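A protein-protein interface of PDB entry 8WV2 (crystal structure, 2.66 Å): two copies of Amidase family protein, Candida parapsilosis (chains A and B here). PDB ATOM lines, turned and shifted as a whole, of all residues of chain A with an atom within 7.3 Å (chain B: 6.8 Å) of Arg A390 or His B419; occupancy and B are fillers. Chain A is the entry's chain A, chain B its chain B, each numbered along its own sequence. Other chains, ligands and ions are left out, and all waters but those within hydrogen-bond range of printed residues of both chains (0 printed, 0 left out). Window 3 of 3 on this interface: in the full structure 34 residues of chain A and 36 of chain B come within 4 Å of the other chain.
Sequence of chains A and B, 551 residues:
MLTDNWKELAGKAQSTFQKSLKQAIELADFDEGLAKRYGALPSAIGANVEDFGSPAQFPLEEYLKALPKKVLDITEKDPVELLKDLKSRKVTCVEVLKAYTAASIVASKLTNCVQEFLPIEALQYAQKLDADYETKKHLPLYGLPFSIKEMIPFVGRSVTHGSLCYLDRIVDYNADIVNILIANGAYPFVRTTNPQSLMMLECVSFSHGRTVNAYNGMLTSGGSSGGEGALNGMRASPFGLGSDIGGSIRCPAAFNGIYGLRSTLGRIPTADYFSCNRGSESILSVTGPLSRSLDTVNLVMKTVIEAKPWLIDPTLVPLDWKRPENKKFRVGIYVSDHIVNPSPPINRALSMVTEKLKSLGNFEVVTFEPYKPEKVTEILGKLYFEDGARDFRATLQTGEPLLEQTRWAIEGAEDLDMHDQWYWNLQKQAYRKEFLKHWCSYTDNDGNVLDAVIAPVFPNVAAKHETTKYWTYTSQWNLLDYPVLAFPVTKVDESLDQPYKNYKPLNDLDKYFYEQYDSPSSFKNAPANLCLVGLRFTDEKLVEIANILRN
The indole nitrogen (NE1) of Trp B422 lies within hydrogen-bond range of the side-chain carboxylate (OE2) of Glu A386 (2.9 Å). The side-chain carboxylate of Asp A387 is in hydrogen-bond range of a ring nitrogen (NE2) of His B419 (2.6 Å). NH2 of Arg A390 lies within salt-bridge range of OD2 of Asp B417, 2.9 Å away. ND1 of His B419 sits at hydrogen-bond distance from NH2 of Arg A390, 3.4 Å away. SD of Met A418 lies close to NE2 of Gln B421, 3.5 Å away.
N of Asn A277 is in hydrogen-bond range of OD2 of Asp A391 (2.9 Å). The backbone carbonyl oxygen (O) of Glu A386 sits at hydrogen-bond distance from the backbone NH (N) of Leu A416, 2.9 Å away. The backbone NH (N) of Arg A390 is in hydrogen-bond range of the side-chain carboxylate (OD1) of Asp A387 (3.3 Å). The backbone NH (N) of Asp A391 sits at hydrogen-bond distance from the side-chain carboxylate (OD2) of Asp A387 (2.7 Å). N of His B419 sits at hydrogen-bond distance from OD2 of Asp B417 (2.7 Å). N of Asp B417 is in hydrogen-bond range of OD2 of Asp B420 (3.4 Å).
Among the printed residues, pairs that only touch across the chains: Arg A278 with Trp B422 (3.2 Å), Leu A416 with Met B418 (3.2 Å), Glu A386 with Met B418 (3.2 Å), Asn A277 with Trp B422 (3.3 Å), Asp A387 with Trp B422 (3.3 Å), Gly A279 with Trp B422 (3.5 Å), Met A418 with Met B418 (3.6 Å), Met A418 with Leu B416 (3.6 Å) and Asp A391 with Trp B422 (3.9 Å).
Printed residues of chain B within 4 Å of Asn A277: Trp B422. Of the printed residues of chain B, Asp A387 touches His B419 and Trp B422. Ile A410 touches none of the printed residues of chain B. Ala A413 touches none of the printed residues of chain B. Printed residues of chain B within 4 Å of Met A418: Leu B416 (3.6 Å), Met B418 (3.6 Å) and Gln B421 (3.2 Å). Of the printed residues of chain A, Met B418 touches Glu A386 (3.2 Å), Leu A416 (3.2 Å) and Met A418 (3.6 Å). Of chain A, only Asp A387 (2.6 Å) and Arg A390 (3.4 Å) come within 4 Å of His B419. The nearest residue of chain B that does not touch Arg A390 is Met B418 (5.3 Å).
Of the 9 printed residues of chain B, 6 touch a printed residue of chain A. Hydrophobic or aromatic side chains of chain B within 4 Å of the printed part of chain A: Met B418, His B419 and Trp B422. Printed residues of chain A that touch a printed residue of chain B: Asn A277, Arg A278, Gly A279, Glu A386, Asp A387, Arg A390, Asp A391, Leu A416 and Met A418. Hydrophobic or aromatic side chains of chain A that line the printed part of chain B: Met A418. Among the printed residues, Asp or Glu carboxylates within 4 Å of a Lys or Arg side-chain nitrogen of the other chain: Arg A390 with Asp B417 (2.9 Å).
Leu A416 touches Met B418, and with the chains exchanged Met A418 touches Leu B416. Met B418 touches its own counterpart, Met A418. 2 positions are printed for both chains.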
ATOM      1  N   ASN A 277     -16.977 -21.879  -2.323  1.00  0.00           N
ATOM      2  CA  ASN A 277     -17.980 -22.857  -2.748  1.00  0.00           C
ATOM      3  C   ASN A 277     -18.235 -23.906  -1.664  1.00  0.00           C
ATOM      4  O   ASN A 277     -18.236 -25.115  -1.911  1.00  0.00           O
ATOM      5  CB  ASN A 277     -17.584 -23.513  -4.070  1.00  0.00           C
ATOM      6  CG  ASN A 277     -17.027 -22.521  -5.076  1.00  0.00           C
ATOM      7  OD1 ASN A 277     -16.032 -22.810  -5.732  1.00  0.00           O
ATOM      8  ND2 ASN A 277     -17.674 -21.361  -5.220  1.00  0.00           N
ATOM      9  N   ARG A 278     -18.425 -23.427  -0.441  1.00  0.00           N
ATOM     10  CA  ARG A 278     -18.706 -24.306   0.683  1.00  0.00           C
ATOM     11  C   ARG A 278     -20.069 -24.958   0.494  1.00  0.00           C
ATOM     12  O   ARG A 278     -21.071 -24.281   0.247  1.00  0.00           O
ATOM     13  CB  ARG A 278     -18.663 -23.504   1.978  1.00  0.00           C
ATOM     14  CG  ARG A 278     -17.263 -23.031   2.339  1.00  0.00           C
ATOM     15  CD  ARG A 278     -17.222 -22.378   3.703  1.00  0.00           C
ATOM     16  NE  ARG A 278     -17.974 -21.133   3.636  1.00  0.00           N
ATOM     17  CZ  ARG A 278     -18.348 -20.395   4.678  1.00  0.00           C
ATOM     18  NH1 ARG A 278     -19.033 -19.280   4.455  1.00  0.00           N
ATOM     19  NH2 ARG A 278     -18.031 -20.747   5.924  1.00  0.00           N
ATOM     20  N   GLY A 279     -20.110 -26.278   0.621  1.00  0.00           N
ATOM     21  CA  GLY A 279     -21.295 -27.033   0.299  1.00  0.00           C
ATOM     22  C   GLY A 279     -21.307 -27.614  -1.099  1.00  0.00           C
ATOM     23  O   GLY A 279     -22.145 -28.479  -1.380  1.00  0.00           O
ATOM     24  N   PHE A 385     -16.688 -24.338 -10.485  1.00  0.00           N
ATOM     25  CA  PHE A 385     -17.460 -23.164 -10.072  1.00  0.00           C
ATOM     26  C   PHE A 385     -18.885 -23.327 -10.589  1.00  0.00           C
ATOM     27  O   PHE A 385     -19.268 -22.685 -11.571  1.00  0.00           O
ATOM     28  CB  PHE A 385     -16.821 -21.890 -10.619  1.00  0.00           C
ATOM     29  CG  PHE A 385     -15.574 -21.477  -9.909  1.00  0.00           C
ATOM     30  CD1 PHE A 385     -15.645 -20.790  -8.712  1.00  0.00           C
ATOM     31  CD2 PHE A 385     -14.331 -21.771 -10.439  1.00  0.00           C
ATOM     32  CE1 PHE A 385     -14.493 -20.397  -8.054  1.00  0.00           C
ATOM     33  CE2 PHE A 385     -13.175 -21.382  -9.785  1.00  0.00           C
ATOM     34  CZ  PHE A 385     -13.261 -20.695  -8.591  1.00  0.00           C
ATOM     35  N   GLU A 386     -19.680 -24.158  -9.910  1.00  0.00           N
ATOM     36  CA  GLU A 386     -21.007 -24.504 -10.415  1.00  0.00           C
ATOM     37  C   GLU A 386     -22.046 -23.426 -10.134  1.00  0.00           C
ATOM     38  O   GLU A 386     -23.172 -23.534 -10.625  1.00  0.00           O
ATOM     39  CB  GLU A 386     -21.478 -25.845  -9.839  1.00  0.00           C
ATOM     40  CG  GLU A 386     -21.337 -26.001  -8.332  1.00  0.00           C
ATOM     41  CD  GLU A 386     -21.796 -27.374  -7.853  1.00  0.00           C
ATOM     42  OE1 GLU A 386     -21.998 -28.264  -8.705  1.00  0.00           O
ATOM     43  OE2 GLU A 386     -21.954 -27.565  -6.630  1.00  0.00           O
ATOM     44  N   ASP A 387     -21.703 -22.394  -9.363  1.00  0.00           N
ATOM     45  CA  ASP A 387     -22.595 -21.266  -9.135  1.00  0.00           C
ATOM     46  C   ASP A 387     -22.259 -20.082 -10.034  1.00  0.00           C
ATOM     47  O   ASP A 387     -22.667 -18.949  -9.740  1.00  0.00           O
ATOM     48  CB  ASP A 387     -22.558 -20.833  -7.665  1.00  0.00           C
ATOM     49  CG  ASP A 387     -21.260 -20.116  -7.285  1.00  0.00           C
ATOM     50  OD1 ASP A 387     -20.228 -20.305  -7.970  1.00  0.00           O
ATOM     51  OD2 ASP A 387     -21.285 -19.359  -6.292  1.00  0.00           O
ATOM     52  N   GLY A 388     -21.511 -20.314 -11.107  1.00  0.00           N
ATOM     53  CA  GLY A 388     -21.068 -19.214 -11.939  1.00  0.00           C
ATOM     54  C   GLY A 388     -20.078 -18.301 -11.258  1.00  0.00           C
ATOM     55  O   GLY A 388     -19.998 -17.116 -11.604  1.00  0.00           O
ATOM     56  N   ALA A 389     -19.329 -18.823 -10.284  1.00  0.00           N
ATOM     57  CA  ALA A 389     -18.339 -18.071  -9.518  1.00  0.00           C
ATOM     58  C   ALA A 389     -18.964 -16.939  -8.710  1.00  0.00           C
ATOM     59  O   ALA A 389     -18.280 -15.969  -8.370  1.00  0.00           O
ATOM     60  CB  ALA A 389     -17.226 -17.522 -10.424  1.00  0.00           C
ATOM     61  N   ARG A 390     -20.261 -17.024  -8.403  1.00  0.00           N
ATOM     62  CA  ARG A 390     -20.878 -15.966  -7.611  1.00  0.00           C
ATOM     63  C   ARG A 390     -20.270 -15.904  -6.214  1.00  0.00           C
ATOM     64  O   ARG A 390     -20.024 -14.813  -5.686  1.00  0.00           O
ATOM     65  CB  ARG A 390     -22.394 -16.148  -7.524  1.00  0.00           C
ATOM     66  CG  ARG A 390     -23.122 -15.821  -8.817  1.00  0.00           C
ATOM     67  CD  ARG A 390     -24.641 -15.794  -8.656  1.00  0.00           C
ATOM     68  NE  ARG A 390     -25.254 -17.006  -8.126  1.00  0.00           N
ATOM     69  CZ  ARG A 390     -26.354 -16.995  -7.380  1.00  0.00           C
ATOM     70  NH1 ARG A 390     -26.937 -15.839  -7.086  1.00  0.00           N
ATOM     71  NH2 ARG A 390     -26.870 -18.130  -6.921  1.00  0.00           N
ATOM     72  N   ASP A 391     -20.028 -17.066  -5.596  1.00  0.00           N
ATOM     73  CA  ASP A 391     -19.483 -17.072  -4.244  1.00  0.00           C
ATOM     74  C   ASP A 391     -18.094 -16.454  -4.207  1.00  0.00           C
ATOM     75  O   ASP A 391     -17.773 -15.692  -3.287  1.00  0.00           O
ATOM     76  CB  ASP A 391     -19.445 -18.484  -3.678  1.00  0.00           C
ATOM     77  CG  ASP A 391     -18.895 -18.517  -2.265  1.00  0.00           C
ATOM     78  OD1 ASP A 391     -19.528 -17.933  -1.360  1.00  0.00           O
ATOM     79  OD2 ASP A 391     -17.815 -19.105  -2.064  1.00  0.00           O
ATOM     80  N   PHE A 392     -17.244 -16.782  -5.181  1.00  0.00           N
ATOM     81  CA  PHE A 392     -15.924 -16.169  -5.190  1.00  0.00           C
ATOM     82  C   PHE A 392     -16.015 -14.674  -5.476  1.00  0.00           C
ATOM     83  O   PHE A 392     -15.385 -13.867  -4.780  1.00  0.00           O
ATOM     84  CB  PHE A 392     -14.997 -16.827  -6.203  1.00  0.00           C
ATOM     85  CG  PHE A 392     -13.751 -16.029  -6.432  1.00  0.00           C
ATOM     86  CD1 PHE A 392     -12.814 -15.907  -5.428  1.00  0.00           C
ATOM     87  CD2 PHE A 392     -13.546 -15.347  -7.618  1.00  0.00           C
ATOM     88  CE1 PHE A 392     -11.684 -15.150  -5.616  1.00  0.00           C
ATOM     89  CE2 PHE A 392     -12.412 -14.592  -7.807  1.00  0.00           C
ATOM     90  CZ  PHE A 392     -11.485 -14.492  -6.807  1.00  0.00           C
ATOM     91  N   ARG A 393     -16.781 -14.281  -6.502  1.00  0.00           N
ATOM     92  CA  ARG A 393     -16.810 -12.865  -6.868  1.00  0.00           C
ATOM     93  C   ARG A 393     -17.325 -12.000  -5.728  1.00  0.00           C
ATOM     94  O   ARG A 393     -16.948 -10.827  -5.619  1.00  0.00           O
ATOM     95  CB  ARG A 393     -17.644 -12.633  -8.128  1.00  0.00           C
ATOM     96  CG  ARG A 393     -17.015 -13.179  -9.384  1.00  0.00           C
ATOM     97  CD  ARG A 393     -17.808 -12.751 -10.597  1.00  0.00           C
ATOM     98  NE  ARG A 393     -16.972 -12.668 -11.790  1.00  0.00           N
ATOM     99  CZ  ARG A 393     -17.041 -13.526 -12.801  1.00  0.00           C
ATOM    100  NH1 ARG A 393     -17.920 -14.515 -12.764  1.00  0.00           N
ATOM    101  NH2 ARG A 393     -16.243 -13.392 -13.852  1.00  0.00           N
ATOM    102  N   ALA A 394     -18.166 -12.562  -4.861  1.00  0.00           N
ATOM    103  CA  ALA A 394     -18.624 -11.802  -3.709  1.00  0.00           C
ATOM    104  C   ALA A 394     -17.481 -11.434  -2.771  1.00  0.00           C
ATOM    105  O   ALA A 394     -17.633 -10.503  -1.972  1.00  0.00           O
ATOM    106  CB  ALA A 394     -19.699 -12.590  -2.956  1.00  0.00           C
ATOM    107  N   THR A 395     -16.344 -12.140  -2.836  1.00  0.00           N
ATOM    108  CA  THR A 395     -15.191 -11.758  -2.018  1.00  0.00           C
ATOM    109  C   THR A 395     -14.538 -10.466  -2.500  1.00  0.00           C
ATOM    110  O   THR A 395     -13.814  -9.833  -1.726  1.00  0.00           O
ATOM    111  CB  THR A 395     -14.134 -12.872  -1.983  1.00  0.00           C
ATOM    112  OG1 THR A 395     -13.568 -13.060  -3.288  1.00  0.00           O
ATOM    113  CG2 THR A 395     -14.742 -14.192  -1.502  1.00  0.00           C
ATOM    114  N   GLN A 397     -15.979  -7.652  -3.238  1.00  0.00           N
ATOM    115  CA  GLN A 397     -16.725  -6.453  -2.871  1.00  0.00           C
ATOM    116  C   GLN A 397     -15.872  -5.474  -2.083  1.00  0.00           C
ATOM    117  O   GLN A 397     -16.217  -4.293  -1.985  1.00  0.00           O
ATOM    118  CB  GLN A 397     -17.962  -6.862  -2.078  1.00  0.00           C
ATOM    119  CG  GLN A 397     -18.931  -7.693  -2.896  1.00  0.00           C
ATOM    120  CD  GLN A 397     -20.238  -7.940  -2.175  1.00  0.00           C
ATOM    121  OE1 GLN A 397     -20.555  -7.270  -1.189  1.00  0.00           O
ATOM    122  NE2 GLN A 397     -21.015  -8.900  -2.673  1.00  0.00           N
ATOM    123  N   ILE A 410     -12.152 -18.785 -13.312  1.00  0.00           N
ATOM    124  CA  ILE A 410     -13.571 -18.433 -13.283  1.00  0.00           C
ATOM    125  C   ILE A 410     -14.111 -18.040 -14.647  1.00  0.00           C
ATOM    126  O   ILE A 410     -15.334 -17.876 -14.792  1.00  0.00           O
ATOM    127  CB  ILE A 410     -13.856 -17.305 -12.266  1.00  0.00           C
ATOM    128  CG1 ILE A 410     -13.115 -16.024 -12.655  1.00  0.00           C
ATOM    129  CG2 ILE A 410     -13.523 -17.750 -10.856  1.00  0.00           C
ATOM    130  CD1 ILE A 410     -13.430 -14.837 -11.764  1.00  0.00           C
ATOM    131  N   ALA A 413     -17.432 -19.747 -16.218  1.00  0.00           N
ATOM    132  CA  ALA A 413     -18.216 -20.423 -15.193  1.00  0.00           C
ATOM    133  C   ALA A 413     -19.699 -20.116 -15.351  1.00  0.00           C
ATOM    134  O   ALA A 413     -20.102 -18.949 -15.394  1.00  0.00           O
ATOM    135  CB  ALA A 413     -17.743 -20.008 -13.799  1.00  0.00           C
ATOM    136  N   GLU A 414     -20.507 -21.173 -15.421  1.00  0.00           N
ATOM    137  CA  GLU A 414     -21.958 -21.067 -15.488  1.00  0.00           C
ATOM    138  C   GLU A 414     -22.585 -21.258 -14.112  1.00  0.00           C
ATOM    139  O   GLU A 414     -22.089 -22.031 -13.289  1.00  0.00           O
ATOM    140  CB  GLU A 414     -22.545 -22.092 -16.466  1.00  0.00           C
ATOM    141  CG  GLU A 414     -22.223 -21.854 -17.937  1.00  0.00           C
ATOM    142  CD  GLU A 414     -23.027 -22.765 -18.846  1.00  0.00           C
ATOM    143  OE1 GLU A 414     -23.808 -23.589 -18.316  1.00  0.00           O
ATOM    144  OE2 GLU A 414     -22.899 -22.641 -20.085  1.00  0.00           O
ATOM    145  N   ASP A 415     -23.666 -20.523 -13.865  1.00  0.00           N
ATOM    146  CA  ASP A 415     -24.512 -20.722 -12.692  1.00  0.00           C
ATOM    147  C   ASP A 415     -25.509 -21.817 -13.047  1.00  0.00           C
ATOM    148  O   ASP A 415     -26.543 -21.560 -13.666  1.00  0.00           O
ATOM    149  CB  ASP A 415     -25.203 -19.418 -12.307  1.00  0.00           C
ATOM    150  CG  ASP A 415     -25.939 -19.501 -10.984  1.00  0.00           C
ATOM    151  OD1 ASP A 415     -25.801 -20.525 -10.281  1.00  0.00           O
ATOM    152  OD2 ASP A 415     -26.646 -18.531 -10.636  1.00  0.00           O
ATOM    153  N   LEU A 416     -25.183 -23.052 -12.676  1.00  0.00           N
ATOM    154  CA  LEU A 416     -25.945 -24.211 -13.125  1.00  0.00           C
ATOM    155  C   LEU A 416     -27.300 -24.306 -12.430  1.00  0.00           C
ATOM    156  O   LEU A 416     -27.399 -24.173 -11.205  1.00  0.00           O
ATOM    157  CB  LEU A 416     -25.156 -25.491 -12.873  1.00  0.00           C
ATOM    158  CG  LEU A 416     -23.772 -25.635 -13.508  1.00  0.00           C
ATOM    159  CD1 LEU A 416     -23.179 -26.996 -13.162  1.00  0.00           C
ATOM    160  CD2 LEU A 416     -23.826 -25.434 -15.013  1.00  0.00           C
ATOM    161  N   MET A 418     -30.322 -26.982 -11.435  1.00  0.00           N
ATOM    162  CA  MET A 418     -30.222 -28.360 -10.934  1.00  0.00           C
ATOM    163  C   MET A 418     -30.062 -29.382 -12.055  1.00  0.00           C
ATOM    164  O   MET A 418     -29.245 -30.303 -11.954  1.00  0.00           O
ATOM    165  CB  MET A 418     -31.443 -28.719 -10.088  1.00  0.00           C
ATOM    166  CG  MET A 418     -31.277 -28.488  -8.596  1.00  0.00           C
ATOM    167  SD  MET A 418     -29.902 -29.419  -7.860  1.00  0.00           S
ATOM    168  CE  MET A 418     -29.061 -28.067  -7.051  1.00  0.00           C
ATOM    169  N   LEU B 416     -34.006 -25.873  -6.140  1.00  0.00           N
ATOM    170  CA  LEU B 416     -32.909 -25.261  -5.404  1.00  0.00           C
ATOM    171  C   LEU B 416     -31.933 -24.565  -6.341  1.00  0.00           C
ATOM    172  O   LEU B 416     -31.528 -25.116  -7.371  1.00  0.00           O
ATOM    173  CB  LEU B 416     -32.169 -26.300  -4.570  1.00  0.00           C
ATOM    174  CG  LEU B 416     -32.965 -27.077  -3.522  1.00  0.00           C
ATOM    175  CD1 LEU B 416     -32.050 -28.023  -2.768  1.00  0.00           C
ATOM    176  CD2 LEU B 416     -33.695 -26.148  -2.562  1.00  0.00           C
ATOM    177  N   ASP B 417     -31.573 -23.338  -5.978  1.00  0.00           N
ATOM    178  CA  ASP B 417     -30.405 -22.692  -6.544  1.00  0.00           C
ATOM    179  C   ASP B 417     -29.152 -23.386  -6.015  1.00  0.00           C
ATOM    180  O   ASP B 417     -29.165 -23.999  -4.943  1.00  0.00           O
ATOM    181  CB  ASP B 417     -30.419 -21.207  -6.171  1.00  0.00           C
ATOM    182  CG  ASP B 417     -29.211 -20.455  -6.666  1.00  0.00           C
ATOM    183  OD1 ASP B 417     -29.385 -19.654  -7.609  1.00  0.00           O
ATOM    184  OD2 ASP B 417     -28.093 -20.661  -6.142  1.00  0.00           O
ATOM    185  N   MET B 418     -28.064 -23.299  -6.784  1.00  0.00           N
ATOM    186  CA  MET B 418     -26.805 -23.934  -6.390  1.00  0.00           C
ATOM    187  C   MET B 418     -26.431 -23.584  -4.951  1.00  0.00           C
ATOM    188  O   MET B 418     -25.968 -24.441  -4.193  1.00  0.00           O
ATOM    189  CB  MET B 418     -25.691 -23.504  -7.343  1.00  0.00           C
ATOM    190  CG  MET B 418     -25.545 -24.367  -8.586  1.00  0.00           C
ATOM    191  SD  MET B 418     -25.194 -26.099  -8.279  1.00  0.00           S
ATOM    192  CE  MET B 418     -26.498 -26.878  -9.230  1.00  0.00           C
ATOM    193  N   HIS B 419     -26.622 -22.321  -4.559  1.00  0.00           N
ATOM    194  CA  HIS B 419     -26.309 -21.915  -3.193  1.00  0.00           C
ATOM    195  C   HIS B 419     -27.243 -22.569  -2.181  1.00  0.00           C
ATOM    196  O   HIS B 419     -26.811 -22.914  -1.075  1.00  0.00           O
ATOM    197  CB  HIS B 419     -26.382 -20.390  -3.085  1.00  0.00           C
ATOM    198  CG  HIS B 419     -25.289 -19.685  -3.820  1.00  0.00           C
ATOM    199  ND1 HIS B 419     -25.238 -18.314  -3.947  1.00  0.00           N
ATOM    200  CD2 HIS B 419     -24.180 -20.160  -4.438  1.00  0.00           C
ATOM    201  CE1 HIS B 419     -24.161 -17.976  -4.636  1.00  0.00           C
ATOM    202  NE2 HIS B 419     -23.498 -19.078  -4.938  1.00  0.00           N
ATOM    203  N   ASP B 420     -28.510 -22.783  -2.548  1.00  0.00           N
ATOM    204  CA  ASP B 420     -29.419 -23.488  -1.645  1.00  0.00           C
ATOM    205  C   ASP B 420     -28.975 -24.931  -1.442  1.00  0.00           C
ATOM    206  O   ASP B 420     -28.983 -25.438  -0.311  1.00  0.00           O
ATOM    207  CB  ASP B 420     -30.847 -23.418  -2.181  1.00  0.00           C
ATOM    208  CG  ASP B 420     -31.423 -22.020  -2.103  1.00  0.00           C
ATOM    209  OD1 ASP B 420     -31.136 -21.314  -1.110  1.00  0.00           O
ATOM    210  OD2 ASP B 420     -32.120 -21.611  -3.055  1.00  0.00           O
ATOM    211  N   GLN B 421     -28.554 -25.598  -2.519  1.00  0.00           N
ATOM    212  CA  GLN B 421     -28.022 -26.946  -2.371  1.00  0.00           C
ATOM    213  C   GLN B 421     -26.783 -26.936  -1.478  1.00  0.00           C
ATOM    214  O   GLN B 421     -26.614 -27.808  -0.619  1.00  0.00           O
ATOM    215  CB  GLN B 421     -27.717 -27.555  -3.744  1.00  0.00           C
ATOM    216  CG  GLN B 421     -27.217 -28.992  -3.664  1.00  0.00           C
ATOM    217  CD  GLN B 421     -26.716 -29.535  -4.981  1.00  0.00           C
ATOM    218  OE1 GLN B 421     -25.629 -29.191  -5.431  1.00  0.00           O
ATOM    219  NE2 GLN B 421     -27.486 -30.426  -5.586  1.00  0.00           N
ATOM    220  N   TRP B 422     -25.900 -25.957  -1.669  1.00  0.00           N
ATOM    221  CA  TRP B 422     -24.732 -25.849  -0.801  1.00  0.00           C
ATOM    222  C   TRP B 422     -25.141 -25.718   0.663  1.00  0.00           C
ATOM    223  O   TRP B 422     -24.555 -26.367   1.541  1.00  0.00           O
ATOM    224  CB  TRP B 422     -23.872 -24.669  -1.236  1.00  0.00           C
ATOM    225  CG  TRP B 422     -23.264 -24.833  -2.606  1.00  0.00           C
ATOM    226  CD1 TRP B 422     -23.400 -25.900  -3.451  1.00  0.00           C
ATOM    227  CD2 TRP B 422     -22.420 -23.895  -3.280  1.00  0.00           C
ATOM    228  NE1 TRP B 422     -22.691 -25.677  -4.613  1.00  0.00           N
ATOM    229  CE2 TRP B 422     -22.079 -24.455  -4.527  1.00  0.00           C
ATOM    230  CE3 TRP B 422     -21.909 -22.639  -2.943  1.00  0.00           C
ATOM    231  CZ2 TRP B 422     -21.253 -23.799  -5.435  1.00  0.00           C
ATOM    232  CZ3 TRP B 422     -21.094 -21.988  -3.850  1.00  0.00           C
ATOM    233  CH2 TRP B 422     -20.771 -22.570  -5.078  1.00  0.00           C
ATOM    234  N   TYR B 423     -26.138 -24.875   0.946  1.00  0.00           N
ATOM    235  CA  TYR B 423     -26.603 -24.706   2.318  1.00  0.00           C
ATOM    236  C   TYR B 423     -27.094 -26.020   2.905  1.00  0.00           C
ATOM    237  O   TYR B 423     -26.783 -26.353   4.055  1.00  0.00           O
ATOM    238  CB  TYR B 423     -27.722 -23.666   2.377  1.00  0.00           C
ATOM    239  CG  TYR B 423     -28.290 -23.449   3.769  1.00  0.00           C
ATOM    240  CD1 TYR B 423     -27.689 -22.560   4.648  1.00  0.00           C
ATOM    241  CD2 TYR B 423     -29.414 -24.145   4.212  1.00  0.00           C
ATOM    242  CE1 TYR B 423     -28.196 -22.354   5.915  1.00  0.00           C
ATOM    243  CE2 TYR B 423     -29.923 -23.945   5.484  1.00  0.00           C
ATOM    244  CZ  TYR B 423     -29.309 -23.045   6.328  1.00  0.00           C
ATOM    245  OH  TYR B 423     -29.801 -22.829   7.594  1.00  0.00           O
ATOM    246  N   TRP B 424     -27.869 -26.778   2.136  1.00  0.00           N
ATOM    247  CA  TRP B 424     -28.463 -27.983   2.702  1.00  0.00           C
ATOM    248  C   TRP B 424     -27.507 -29.166   2.674  1.00  0.00           C
ATOM    249  O   TRP B 424     -27.627 -30.063   3.515  1.00  0.00           O
ATOM    250  CB  TRP B 424     -29.772 -28.308   1.986  1.00  0.00           C
ATOM    251  CG  TRP B 424     -30.855 -27.323   2.328  1.00  0.00           C
ATOM    252  CD1 TRP B 424     -31.375 -26.348   1.511  1.00  0.00           C
ATOM    253  CD2 TRP B 424     -31.539 -27.199   3.582  1.00  0.00           C
ATOM    254  NE1 TRP B 424     -32.343 -25.637   2.182  1.00  0.00           N
ATOM    255  CE2 TRP B 424     -32.463 -26.138   3.453  1.00  0.00           C
ATOM    256  CE3 TRP B 424     -31.465 -27.883   4.798  1.00  0.00           C
ATOM    257  CZ2 TRP B 424     -33.309 -25.755   4.498  1.00  0.00           C
ATOM    258  CZ3 TRP B 424     -32.309 -27.501   5.834  1.00  0.00           C
ATOM    259  CH2 TRP B 424     -33.216 -26.448   5.674  1.00  0.00           C
